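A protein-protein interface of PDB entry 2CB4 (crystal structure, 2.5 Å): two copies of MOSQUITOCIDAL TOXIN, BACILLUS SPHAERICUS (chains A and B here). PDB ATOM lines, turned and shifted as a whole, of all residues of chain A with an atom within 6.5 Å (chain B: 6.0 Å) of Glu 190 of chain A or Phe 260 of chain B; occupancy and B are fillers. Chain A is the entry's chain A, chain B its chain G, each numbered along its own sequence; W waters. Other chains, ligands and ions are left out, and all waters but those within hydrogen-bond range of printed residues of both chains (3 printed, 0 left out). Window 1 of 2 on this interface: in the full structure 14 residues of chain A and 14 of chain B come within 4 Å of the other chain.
Water W2 lies within hydrogen-bond range of OE2 of Glu 190 of chain A (2.6 Å), O of Arg 116 of chain B (2.7 Å) and NH2 of Arg 188 of chain A (2.9 Å).
Water W3 lies within hydrogen-bond range of the backbone carbonyl oxygen of Pro 262 of chain B (2.6 Å) and the backbone carbonyl oxygen of Phe 212 of chain A (2.9 Å).
Water W1 bridges O of Thr 117 of chain B (2.7 Å) and OE1 of Glu 190 of chain A (2.8 Å).
No position is printed for both chains.
Hydrophobic or aromatic side chains of chain B within 4 Å of the printed part of chain A: Phe 175, Phe 257, Phe 260 and Pro 262.
Along chain B the printed residues that touch a printed residue of chain A span positions 116 to 263.
Of the 16 printed residues of chain A, 5 touch a printed residue of chain B.
Printed residues of chain A that touch a printed residue of chain B: Phe 90, Arg 188, Glu 190, Asn 211 and Ile 213.
Phe 260 of chain B touches one residue of chain A.
Of the printed residues of chain A, Arg 116 of chain B touches Glu 190.
Printed residues of chain B within 4 Å of Phe 90 of chain A: Phe 257 (3.9 Å).
Asn 209 of chain A touches none of the printed residues of chain B.
Phe 212 of chain A touches none of the printed residues of chain B.
The nearest residue of chain A that does not touch Phe 260 of chain B is Arg 188 of chain A (5.5 Å).
O of Phe 90 of chain A touches CZ of Phe 257 of chain B, at 3.9 Å.
Thr 117 of chain B touches Arg 188 of chain A.
Arg 116 of chain B touches Glu 190 of chain A (O to OE2, 3.8 Å).
Phe 260 of chain B touches Glu 190 of chain A.
ND2 of Asn 211 of chain A touches CE2 of Phe 257 of chain B, 3.9 Å away.
Asn 211 of chain A touches Pro 262 of chain B (CA to O, 3.3 Å).
OD1 of Asn 263 of chain B touches CB of Asn 211 of chain A, 3.1 Å away.
CE1 of Phe 175 of chain B touches CD1 of Ile 213 of chain A, 3.7 Å away.
The side-chain amide nitrogen of Asn 263 of chain B is in hydrogen-bond range of the backbone carbonyl oxygen of Phe 257 of chain B (2.7 Å).
The guanidinium group of Arg 188 of chain A is in salt-bridge range of the side-chain carboxylate of Glu 190 of chain A, at 2.8 Å.
The backbone carbonyl oxygen (O) of Glu 190 of chain A sits at hydrogen-bond distance from the backbone NH (N) of Ile 213 of chain A, 2.7 Å away.
The backbone NH (N) of Arg 188 of chain A sits at hydrogen-bond distance from the backbone carbonyl oxygen (O) of Ala 26 of chain A, 2.9 Å away.
The side-chain amide oxygen (OD1) of Asn 209 of chain A lies close to the backbone NH (N) of Asn 211 of chain A, at 3.2 Å.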
ATOM      1  N   ALA A  26      39.102  13.704  12.264  1.00  0.00           N
ATOM      2  CA  ALA A  26      37.840  13.796  13.026  1.00  0.00           C
ATOM      3  C   ALA A  26      37.166  15.150  12.775  1.00  0.00           C
ATOM      4  O   ALA A  26      36.029  15.369  13.188  1.00  0.00           O
ATOM      5  CB  ALA A  26      38.107  13.603  14.536  1.00  0.00           C
ATOM      6  N   PHE A  90      25.176  15.578  19.848  1.00  0.00           N
ATOM      7  CA  PHE A  90      25.025  14.341  19.057  1.00  0.00           C
ATOM      8  C   PHE A  90      24.551  14.662  17.643  1.00  0.00           C
ATOM      9  O   PHE A  90      24.587  13.812  16.754  1.00  0.00           O
ATOM     10  CB  PHE A  90      24.049  13.342  19.697  1.00  0.00           C
ATOM     11  CG  PHE A  90      24.601  12.612  20.893  1.00  0.00           C
ATOM     12  CD1 PHE A  90      25.905  12.773  21.287  1.00  0.00           C
ATOM     13  CD2 PHE A  90      23.784  11.770  21.647  1.00  0.00           C
ATOM     14  CE1 PHE A  90      26.395  12.113  22.408  1.00  0.00           C
ATOM     15  CE2 PHE A  90      24.288  11.118  22.770  1.00  0.00           C
ATOM     16  CZ  PHE A  90      25.589  11.282  23.136  1.00  0.00           C
ATOM     17  N   GLY A  93      28.187  17.598  16.723  1.00  0.00           N
ATOM     18  CA  GLY A  93      29.522  17.243  17.151  1.00  0.00           C
ATOM     19  C   GLY A  93      30.113  18.428  17.916  1.00  0.00           C
ATOM     20  O   GLY A  93      29.396  19.321  18.389  1.00  0.00           O
ATOM     21  N   PHE A 157      35.857   8.580  20.822  1.00  0.00           N
ATOM     22  CA  PHE A 157      36.856   7.675  20.202  1.00  0.00           C
ATOM     23  C   PHE A 157      36.941   8.234  18.800  1.00  0.00           C
ATOM     24  O   PHE A 157      36.031   8.087  18.017  1.00  0.00           O
ATOM     25  CB  PHE A 157      36.394   6.219  20.163  1.00  0.00           C
ATOM     26  CG  PHE A 157      36.300   5.578  21.535  1.00  0.00           C
ATOM     27  CD1 PHE A 157      37.445   5.070  22.157  1.00  0.00           C
ATOM     28  CD2 PHE A 157      35.077   5.510  22.210  1.00  0.00           C
ATOM     29  CE1 PHE A 157      37.355   4.468  23.406  1.00  0.00           C
ATOM     30  CE2 PHE A 157      34.989   4.915  23.452  1.00  0.00           C
ATOM     31  CZ  PHE A 157      36.139   4.385  24.051  1.00  0.00           C
ATOM     32  N   ILE A 187      35.504  17.777  16.294  1.00  0.00           N
ATOM     33  CA  ILE A 187      35.153  16.371  16.237  1.00  0.00           C
ATOM     34  C   ILE A 187      33.701  16.164  15.764  1.00  0.00           C
ATOM     35  O   ILE A 187      32.771  16.700  16.350  1.00  0.00           O
ATOM     36  CB  ILE A 187      35.277  15.804  17.681  1.00  0.00           C
ATOM     37  CG1 ILE A 187      36.644  16.171  18.275  1.00  0.00           C
ATOM     38  CG2 ILE A 187      34.957  14.297  17.758  1.00  0.00           C
ATOM     39  CD1 ILE A 187      36.744  15.990  19.784  1.00  0.00           C
ATOM     40  N   ARG A 188      33.513  15.360  14.720  1.00  0.00           N
ATOM     41  CA  ARG A 188      32.177  15.064  14.210  1.00  0.00           C
ATOM     42  C   ARG A 188      31.402  14.163  15.184  1.00  0.00           C
ATOM     43  O   ARG A 188      32.005  13.414  15.945  1.00  0.00           O
ATOM     44  CB  ARG A 188      32.308  14.447  12.832  1.00  0.00           C
ATOM     45  CG  ARG A 188      32.881  15.466  11.835  1.00  0.00           C
ATOM     46  CD  ARG A 188      32.742  14.981  10.393  1.00  0.00           C
ATOM     47  NE  ARG A 188      33.275  13.627  10.196  1.00  0.00           N
ATOM     48  CZ  ARG A 188      34.549  13.341   9.927  1.00  0.00           C
ATOM     49  NH1 ARG A 188      35.444  14.308   9.847  1.00  0.00           N
ATOM     50  NH2 ARG A 188      34.935  12.087   9.750  1.00  0.00           N
ATOM     51  N   PRO A 189      30.065  14.237  15.172  1.00  0.00           N
ATOM     52  CA  PRO A 189      29.259  13.464  16.137  1.00  0.00           C
ATOM     53  C   PRO A 189      29.386  11.949  16.099  1.00  0.00           C
ATOM     54  O   PRO A 189      29.121  11.260  17.104  1.00  0.00           O
ATOM     55  CB  PRO A 189      27.815  13.921  15.833  1.00  0.00           C
ATOM     56  CG  PRO A 189      27.857  14.449  14.433  1.00  0.00           C
ATOM     57  CD  PRO A 189      29.213  15.050  14.265  1.00  0.00           C
ATOM     58  N   GLU A 190      29.755  11.401  14.948  1.00  0.00           N
ATOM     59  CA  GLU A 190      29.889   9.934  14.839  1.00  0.00           C
ATOM     60  C   GLU A 190      31.041   9.365  15.683  1.00  0.00           C
ATOM     61  O   GLU A 190      31.137   8.171  15.872  1.00  0.00           O
ATOM     62  CB  GLU A 190      29.938   9.466  13.370  1.00  0.00           C
ATOM     63  CG  GLU A 190      31.171   9.930  12.578  1.00  0.00           C
ATOM     64  CD  GLU A 190      30.945  11.209  11.826  1.00  0.00           C
ATOM     65  OE1 GLU A 190      30.048  11.983  12.225  1.00  0.00           O
ATOM     66  OE2 GLU A 190      31.686  11.449  10.839  1.00  0.00           O
ATOM     67  N   PHE A 191      31.888  10.238  16.217  1.00  0.00           N
ATOM     68  CA  PHE A 191      33.007   9.843  17.086  1.00  0.00           C
ATOM     69  C   PHE A 191      32.673   9.999  18.582  1.00  0.00           C
ATOM     70  O   PHE A 191      33.534   9.788  19.446  1.00  0.00           O
ATOM     71  CB  PHE A 191      34.238  10.675  16.731  1.00  0.00           C
ATOM     72  CG  PHE A 191      34.669  10.481  15.306  1.00  0.00           C
ATOM     73  CD1 PHE A 191      34.918   9.177  14.826  1.00  0.00           C
ATOM     74  CD2 PHE A 191      34.756  11.553  14.427  1.00  0.00           C
ATOM     75  CE1 PHE A 191      35.270   8.971  13.496  1.00  0.00           C
ATOM     76  CE2 PHE A 191      35.101  11.347  13.103  1.00  0.00           C
ATOM     77  CZ  PHE A 191      35.342  10.043  12.626  1.00  0.00           C
ATOM     78  N   ILE A 192      31.431  10.386  18.873  1.00  0.00           N
ATOM     79  CA  ILE A 192      30.972  10.590  20.243  1.00  0.00           C
ATOM     80  C   ILE A 192      30.035   9.449  20.557  1.00  0.00           C
ATOM     81  O   ILE A 192      28.948   9.331  19.981  1.00  0.00           O
ATOM     82  CB  ILE A 192      30.300  11.991  20.438  1.00  0.00           C
ATOM     83  CG1 ILE A 192      31.115  13.074  19.698  1.00  0.00           C
ATOM     84  CG2 ILE A 192      30.141  12.310  21.921  1.00  0.00           C
ATOM     85  CD1 ILE A 192      30.501  14.480  19.751  1.00  0.00           C
ATOM     86  N   ARG A 193      30.498   8.565  21.431  1.00  0.00           N
ATOM     87  CA  ARG A 193      29.743   7.375  21.754  1.00  0.00           C
ATOM     88  C   ARG A 193      28.608   7.539  22.746  1.00  0.00           C
ATOM     89  O   ARG A 193      27.562   6.915  22.620  1.00  0.00           O
ATOM     90  CB  ARG A 193      30.682   6.247  22.238  1.00  0.00           C
ATOM     91  CG  ARG A 193      29.890   4.921  22.406  1.00  0.00           C
ATOM     92  CD  ARG A 193      30.788   3.722  22.453  1.00  0.00           C
ATOM     93  NE  ARG A 193      31.433   3.618  23.751  1.00  0.00           N
ATOM     94  CZ  ARG A 193      32.266   2.650  24.101  1.00  0.00           C
ATOM     95  NH1 ARG A 193      32.545   1.688  23.253  1.00  0.00           N
ATOM     96  NH2 ARG A 193      32.817   2.643  25.307  1.00  0.00           N
ATOM     97  N   ASN A 209      24.773   7.332  21.815  1.00  0.00           N
ATOM     98  CA  ASN A 209      24.647   7.872  20.454  1.00  0.00           C
ATOM     99  C   ASN A 209      24.573   6.637  19.530  1.00  0.00           C
ATOM    100  O   ASN A 209      25.580   5.987  19.299  1.00  0.00           O
ATOM    101  CB  ASN A 209      25.887   8.688  20.085  1.00  0.00           C
ATOM    102  CG  ASN A 209      25.797   9.280  18.698  1.00  0.00           C
ATOM    103  OD1 ASN A 209      24.785   9.154  18.018  1.00  0.00           O
ATOM    104  ND2 ASN A 209      26.848   9.960  18.283  1.00  0.00           N
ATOM    105  N   ASN A 211      24.394   6.425  16.459  1.00  0.00           N
ATOM    106  CA  ASN A 211      25.138   6.692  15.236  1.00  0.00           C
ATOM    107  C   ASN A 211      26.647   6.695  15.430  1.00  0.00           C
ATOM    108  O   ASN A 211      27.390   7.102  14.552  1.00  0.00           O
ATOM    109  CB  ASN A 211      24.704   8.038  14.636  1.00  0.00           C
ATOM    110  CG  ASN A 211      23.199   8.166  14.542  1.00  0.00           C
ATOM    111  OD1 ASN A 211      22.516   7.238  14.150  1.00  0.00           O
ATOM    112  ND2 ASN A 211      22.689   9.318  14.895  1.00  0.00           N
ATOM    113  N   PHE A 212      27.097   6.238  16.587  1.00  0.00           N
ATOM    114  CA  PHE A 212      28.518   6.160  16.855  1.00  0.00           C
ATOM    115  C   PHE A 212      29.140   5.237  15.752  1.00  0.00           C
ATOM    116  O   PHE A 212      28.570   4.220  15.372  1.00  0.00           O
ATOM    117  CB  PHE A 212      28.746   5.586  18.257  1.00  0.00           C
ATOM    118  CG  PHE A 212      30.202   5.363  18.573  1.00  0.00           C
ATOM    119  CD1 PHE A 212      31.096   6.430  18.567  1.00  0.00           C
ATOM    120  CD2 PHE A 212      30.687   4.081  18.808  1.00  0.00           C
ATOM    121  CE1 PHE A 212      32.452   6.227  18.821  1.00  0.00           C
ATOM    122  CE2 PHE A 212      32.047   3.879  19.075  1.00  0.00           C
ATOM    123  CZ  PHE A 212      32.926   4.952  19.061  1.00  0.00           C
ATOM    124  N   ILE A 213      30.294   5.644  15.243  1.00  0.00           N
ATOM    125  CA  ILE A 213      31.018   4.976  14.179  1.00  0.00           C
ATOM    126  C   ILE A 213      31.135   3.433  14.302  1.00  0.00           C
ATOM    127  O   ILE A 213      31.181   2.741  13.290  1.00  0.00           O
ATOM    128  CB  ILE A 213      32.395   5.637  14.026  1.00  0.00           C
ATOM    129  CG1 ILE A 213      32.907   5.546  12.579  1.00  0.00           C
ATOM    130  CG2 ILE A 213      33.358   5.073  15.068  1.00  0.00           C
ATOM    131  CD1 ILE A 213      31.925   5.928  11.559  1.00  0.00           C
ATOM    132  N   ASN A 214      31.163   2.890  15.524  1.00  0.00           N
ATOM    133  CA  ASN A 214      31.187   1.414  15.748  1.00  0.00           C
ATOM    134  C   ASN A 214      30.067   1.005  16.696  1.00  0.00           C
ATOM    135  O   ASN A 214      30.285   0.848  17.897  1.00  0.00           O
ATOM    136  CB  ASN A 214      32.498   0.946  16.345  1.00  0.00           C
ATOM    137  CG  ASN A 214      32.683  -0.577  16.222  1.00  0.00           C
ATOM    138  OD1 ASN A 214      33.811  -1.058  16.183  1.00  0.00           O
ATOM    139  ND2 ASN A 214      31.576  -1.327  16.134  1.00  0.00           N
ATOM    140  N   TYR B 114      31.912  14.592   1.400  1.00  0.00           N
ATOM    141  CA  TYR B 114      30.466  14.517   1.508  1.00  0.00           C
ATOM    142  C   TYR B 114      30.027  13.177   2.107  1.00  0.00           C
ATOM    143  O   TYR B 114      29.305  13.138   3.118  1.00  0.00           O
ATOM    144  CB  TYR B 114      29.831  14.751   0.169  1.00  0.00           C
ATOM    145  CG  TYR B 114      28.394  14.329   0.157  1.00  0.00           C
ATOM    146  CD1 TYR B 114      27.446  14.999   0.951  1.00  0.00           C
ATOM    147  CD2 TYR B 114      27.969  13.198  -0.614  1.00  0.00           C
ATOM    148  CE1 TYR B 114      26.119  14.572   0.980  1.00  0.00           C
ATOM    149  CE2 TYR B 114      26.674  12.777  -0.601  1.00  0.00           C
ATOM    150  CZ  TYR B 114      25.748  13.458   0.201  1.00  0.00           C
ATOM    151  OH  TYR B 114      24.465  13.032   0.199  1.00  0.00           O
ATOM    152  N   LEU B 115      30.490  12.094   1.473  1.00  0.00           N
ATOM    153  CA  LEU B 115      30.197  10.695   1.864  1.00  0.00           C
ATOM    154  C   LEU B 115      30.708  10.305   3.186  1.00  0.00           C
ATOM    155  O   LEU B 115      30.090   9.507   3.901  1.00  0.00           O
ATOM    156  CB  LEU B 115      30.785   9.721   0.844  1.00  0.00           C
ATOM    157  CG  LEU B 115      30.440   9.883  -0.657  1.00  0.00           C
ATOM    158  CD1 LEU B 115      31.419   9.004  -1.414  1.00  0.00           C
ATOM    159  CD2 LEU B 115      28.941   9.494  -0.965  1.00  0.00           C
ATOM    160  N   ARG B 116      31.860  10.832   3.540  1.00  0.00           N
ATOM    161  CA  ARG B 116      32.478  10.495   4.795  1.00  0.00           C
ATOM    162  C   ARG B 116      32.042  11.313   5.998  1.00  0.00           C
ATOM    163  O   ARG B 116      32.057  10.818   7.128  1.00  0.00           O
ATOM    164  CB  ARG B 116      34.007  10.637   4.665  1.00  0.00           C
ATOM    165  CG  ARG B 116      34.768  10.115   5.920  1.00  0.00           C
ATOM    166  CD  ARG B 116      36.277  10.095   5.720  1.00  0.00           C
ATOM    167  NE  ARG B 116      36.699   9.190   4.650  1.00  0.00           N
ATOM    168  CZ  ARG B 116      36.683   7.860   4.742  1.00  0.00           C
ATOM    169  NH1 ARG B 116      36.251   7.265   5.862  1.00  0.00           N
ATOM    170  NH2 ARG B 116      37.093   7.121   3.712  1.00  0.00           N
ATOM    171  N   THR B 117      31.730  12.582   5.770  1.00  0.00           N
ATOM    172  CA  THR B 117      31.419  13.496   6.856  1.00  0.00           C
ATOM    173  C   THR B 117      30.032  14.118   6.846  1.00  0.00           C
ATOM    174  O   THR B 117      29.599  14.678   7.872  1.00  0.00           O
ATOM    175  CB  THR B 117      32.425  14.687   6.851  1.00  0.00           C
ATOM    176  OG1 THR B 117      32.054  15.608   5.825  1.00  0.00           O
ATOM    177  CG2 THR B 117      33.855  14.229   6.603  1.00  0.00           C
ATOM    178  N   ASN B 118      29.362  14.077   5.689  1.00  0.00           N
ATOM    179  CA  ASN B 118      28.045  14.691   5.531  1.00  0.00           C
ATOM    180  C   ASN B 118      28.078  16.209   5.495  1.00  0.00           C
ATOM    181  O   ASN B 118      27.095  16.858   5.821  1.00  0.00           O
ATOM    182  CB  ASN B 118      27.043  14.228   6.588  1.00  0.00           C
ATOM    183  CG  ASN B 118      25.587  14.255   6.070  1.00  0.00           C
ATOM    184  OD1 ASN B 118      25.327  14.131   4.854  1.00  0.00           O
ATOM    185  ND2 ASN B 118      24.658  14.406   6.989  1.00  0.00           N
ATOM    186  N   TRP B 141      18.413  -0.205   3.591  1.00  0.00           N
ATOM    187  CA  TRP B 141      19.236   0.511   4.549  1.00  0.00           C
ATOM    188  C   TRP B 141      18.181   1.480   5.183  1.00  0.00           C
ATOM    189  O   TRP B 141      17.391   2.125   4.467  1.00  0.00           O
ATOM    190  CB  TRP B 141      20.318   1.309   3.804  1.00  0.00           C
ATOM    191  CG  TRP B 141      21.189   2.140   4.711  1.00  0.00           C
ATOM    192  CD1 TRP B 141      22.418   1.796   5.208  1.00  0.00           C
ATOM    193  CD2 TRP B 141      20.895   3.463   5.233  1.00  0.00           C
ATOM    194  NE1 TRP B 141      22.908   2.820   6.003  1.00  0.00           N
ATOM    195  CE2 TRP B 141      22.005   3.856   6.018  1.00  0.00           C
ATOM    196  CE3 TRP B 141      19.828   4.384   5.047  1.00  0.00           C
ATOM    197  CZ2 TRP B 141      22.058   5.095   6.672  1.00  0.00           C
ATOM    198  CZ3 TRP B 141      19.884   5.615   5.695  1.00  0.00           C
ATOM    199  CH2 TRP B 141      20.980   5.947   6.522  1.00  0.00           C
ATOM    200  N   PHE B 175      31.743   4.487   3.194  1.00  0.00           N
ATOM    201  CA  PHE B 175      30.643   3.698   3.756  1.00  0.00           C
ATOM    202  C   PHE B 175      29.813   2.945   2.724  1.00  0.00           C
ATOM    203  O   PHE B 175      28.735   3.412   2.325  1.00  0.00           O
ATOM    204  CB  PHE B 175      29.728   4.607   4.592  1.00  0.00           C
ATOM    205  CG  PHE B 175      30.445   5.331   5.732  1.00  0.00           C
ATOM    206  CD1 PHE B 175      30.990   4.635   6.846  1.00  0.00           C
ATOM    207  CD2 PHE B 175      30.573   6.741   5.687  1.00  0.00           C
ATOM    208  CE1 PHE B 175      31.629   5.386   7.896  1.00  0.00           C
ATOM    209  CE2 PHE B 175      31.193   7.432   6.674  1.00  0.00           C
ATOM    210  CZ  PHE B 175      31.724   6.809   7.764  1.00  0.00           C
ATOM    211  N   GLU B 178      25.713   1.636   2.859  1.00  0.00           N
ATOM    212  CA  GLU B 178      24.545   2.353   2.448  1.00  0.00           C
ATOM    213  C   GLU B 178      24.052   2.096   1.013  1.00  0.00           C
ATOM    214  O   GLU B 178      22.939   2.456   0.668  1.00  0.00           O
ATOM    215  CB  GLU B 178      24.779   3.829   2.718  1.00  0.00           C
ATOM    216  CG  GLU B 178      23.552   4.624   2.594  1.00  0.00           C
ATOM    217  CD  GLU B 178      23.799   6.054   2.914  1.00  0.00           C
ATOM    218  OE1 GLU B 178      24.860   6.324   3.509  1.00  0.00           O
ATOM    219  OE2 GLU B 178      22.959   6.893   2.550  1.00  0.00           O
ATOM    220  N   ASP B 256      19.674  16.058   5.498  1.00  0.00           N
ATOM    221  CA  ASP B 256      20.370  14.795   5.160  1.00  0.00           C
ATOM    222  C   ASP B 256      20.822  13.991   6.377  1.00  0.00           C
ATOM    223  O   ASP B 256      21.552  13.027   6.236  1.00  0.00           O
ATOM    224  CB  ASP B 256      21.633  15.047   4.307  1.00  0.00           C
ATOM    225  CG  ASP B 256      21.333  15.693   2.969  1.00  0.00           C
ATOM    226  OD1 ASP B 256      20.175  15.594   2.496  1.00  0.00           O
ATOM    227  OD2 ASP B 256      22.268  16.295   2.389  1.00  0.00           O
ATOM    228  N   PHE B 257      20.419  14.385   7.576  1.00  0.00           N
ATOM    229  CA  PHE B 257      20.874  13.667   8.755  1.00  0.00           C
ATOM    230  C   PHE B 257      20.550  12.178   8.688  1.00  0.00           C
ATOM    231  O   PHE B 257      21.369  11.326   9.028  1.00  0.00           O
ATOM    232  CB  PHE B 257      20.307  14.307  10.040  1.00  0.00           C
ATOM    233  CG  PHE B 257      21.011  13.858  11.303  1.00  0.00           C
ATOM    234  CD1 PHE B 257      22.281  14.364  11.632  1.00  0.00           C
ATOM    235  CD2 PHE B 257      20.430  12.892  12.137  1.00  0.00           C
ATOM    236  CE1 PHE B 257      22.949  13.935  12.781  1.00  0.00           C
ATOM    237  CE2 PHE B 257      21.084  12.467  13.304  1.00  0.00           C
ATOM    238  CZ  PHE B 257      22.339  12.989  13.631  1.00  0.00           C
ATOM    239  N   ASP B 258      19.337  11.867   8.258  1.00  0.00           N
ATOM    240  CA  ASP B 258      18.883  10.488   8.164  1.00  0.00           C
ATOM    241  C   ASP B 258      19.321   9.703   6.924  1.00  0.00           C
ATOM    242  O   ASP B 258      18.843   8.614   6.690  1.00  0.00           O
ATOM    243  CB  ASP B 258      17.367  10.436   8.333  1.00  0.00           C
ATOM    244  CG  ASP B 258      16.953  10.670   9.780  1.00  0.00           C
ATOM    245  OD1 ASP B 258      17.593  10.065  10.688  1.00  0.00           O
ATOM    246  OD2 ASP B 258      16.078  11.532   9.996  1.00  0.00           O
ATOM    247  N   MET B 259      20.238  10.273   6.147  1.00  0.00           N
ATOM    248  CA  MET B 259      20.772   9.624   4.958  1.00  0.00           C
ATOM    249  C   MET B 259      22.318   9.526   5.007  1.00  0.00           C
ATOM    250  O   MET B 259      22.938   9.194   4.017  1.00  0.00           O
ATOM    251  CB  MET B 259      20.307  10.270   3.631  1.00  0.00           C
ATOM    252  CG  MET B 259      18.902   9.857   3.185  1.00  0.00           C
ATOM    253  SD  MET B 259      18.549   8.017   2.910  1.00  0.00           S
ATOM    254  CE  MET B 259      19.482   8.044   1.304  1.00  0.00           C
ATOM    255  N   PHE B 260      22.918   9.843   6.153  1.00  0.00           N
ATOM    256  CA  PHE B 260      24.366   9.787   6.344  1.00  0.00           C
ATOM    257  C   PHE B 260      24.624   8.350   6.803  1.00  0.00           C
ATOM    258  O   PHE B 260      23.939   7.846   7.696  1.00  0.00           O
ATOM    259  CB  PHE B 260      24.792  10.787   7.430  1.00  0.00           C
ATOM    260  CG  PHE B 260      26.279  10.810   7.684  1.00  0.00           C
ATOM    261  CD1 PHE B 260      27.180  10.674   6.615  1.00  0.00           C
ATOM    262  CD2 PHE B 260      26.777  10.952   8.974  1.00  0.00           C
ATOM    263  CE1 PHE B 260      28.555  10.675   6.836  1.00  0.00           C
ATOM    264  CE2 PHE B 260      28.155  10.963   9.223  1.00  0.00           C
ATOM    265  CZ  PHE B 260      29.048  10.821   8.154  1.00  0.00           C
ATOM    266  N   ALA B 261      25.589   7.677   6.177  1.00  0.00           N
ATOM    267  CA  ALA B 261      25.857   6.267   6.481  1.00  0.00           C
ATOM    268  C   ALA B 261      25.907   5.795   7.928  1.00  0.00           C
ATOM    269  O   ALA B 261      25.222   4.833   8.280  1.00  0.00           O
ATOM    270  CB  ALA B 261      26.994   5.702   5.635  1.00  0.00           C
ATOM    271  N   PRO B 262      26.700   6.452   8.775  1.00  0.00           N
ATOM    272  CA  PRO B 262      26.778   6.061  10.193  1.00  0.00           C
ATOM    273  C   PRO B 262      25.428   6.265  10.942  1.00  0.00           C
ATOM    274  O   PRO B 262      25.244   5.741  12.055  1.00  0.00           O
ATOM    275  CB  PRO B 262      27.850   7.006  10.774  1.00  0.00           C
ATOM    276  CG  PRO B 262      28.570   7.579   9.640  1.00  0.00           C
ATOM    277  CD  PRO B 262      27.672   7.514   8.435  1.00  0.00           C
ATOM    278  N   ASN B 263      24.502   7.024  10.332  1.00  0.00           N
ATOM    279  CA  ASN B 263      23.192   7.311  10.928  1.00  0.00           C
ATOM    280  C   ASN B 263      22.113   6.292  10.634  1.00  0.00           C
ATOM    281  O   ASN B 263      20.923   6.519  10.924  1.00  0.00           O
ATOM    282  CB  ASN B 263      22.714   8.729  10.584  1.00  0.00           C
ATOM    283  CG  ASN B 263      23.616   9.786  11.168  1.00  0.00           C
ATOM    284  OD1 ASN B 263      24.551   9.482  11.904  1.00  0.00           O
ATOM    285  ND2 ASN B 263      23.354  11.023  10.842  1.00  0.00           N
ATOM    286  N   GLY B 264      22.527   5.152  10.078  1.00  0.00           N
ATOM    287  CA  GLY B 264      21.585   4.072   9.779  1.00  0.00           C
ATOM    288  C   GLY B 264      22.331   2.781   9.472  1.00  0.00           C
ATOM    289  O   GLY B 264      23.548   2.697   9.631  1.00  0.00           O
HETATM  290  O   HOH W   1      29.093  13.933  10.388  1.00  0.00           O
HETATM  291  O   HOH W   2      33.160   9.864   9.458  1.00  0.00           O
HETATM  292  O   HOH W   3      26.823   3.889  13.045  1.00  0.00           O
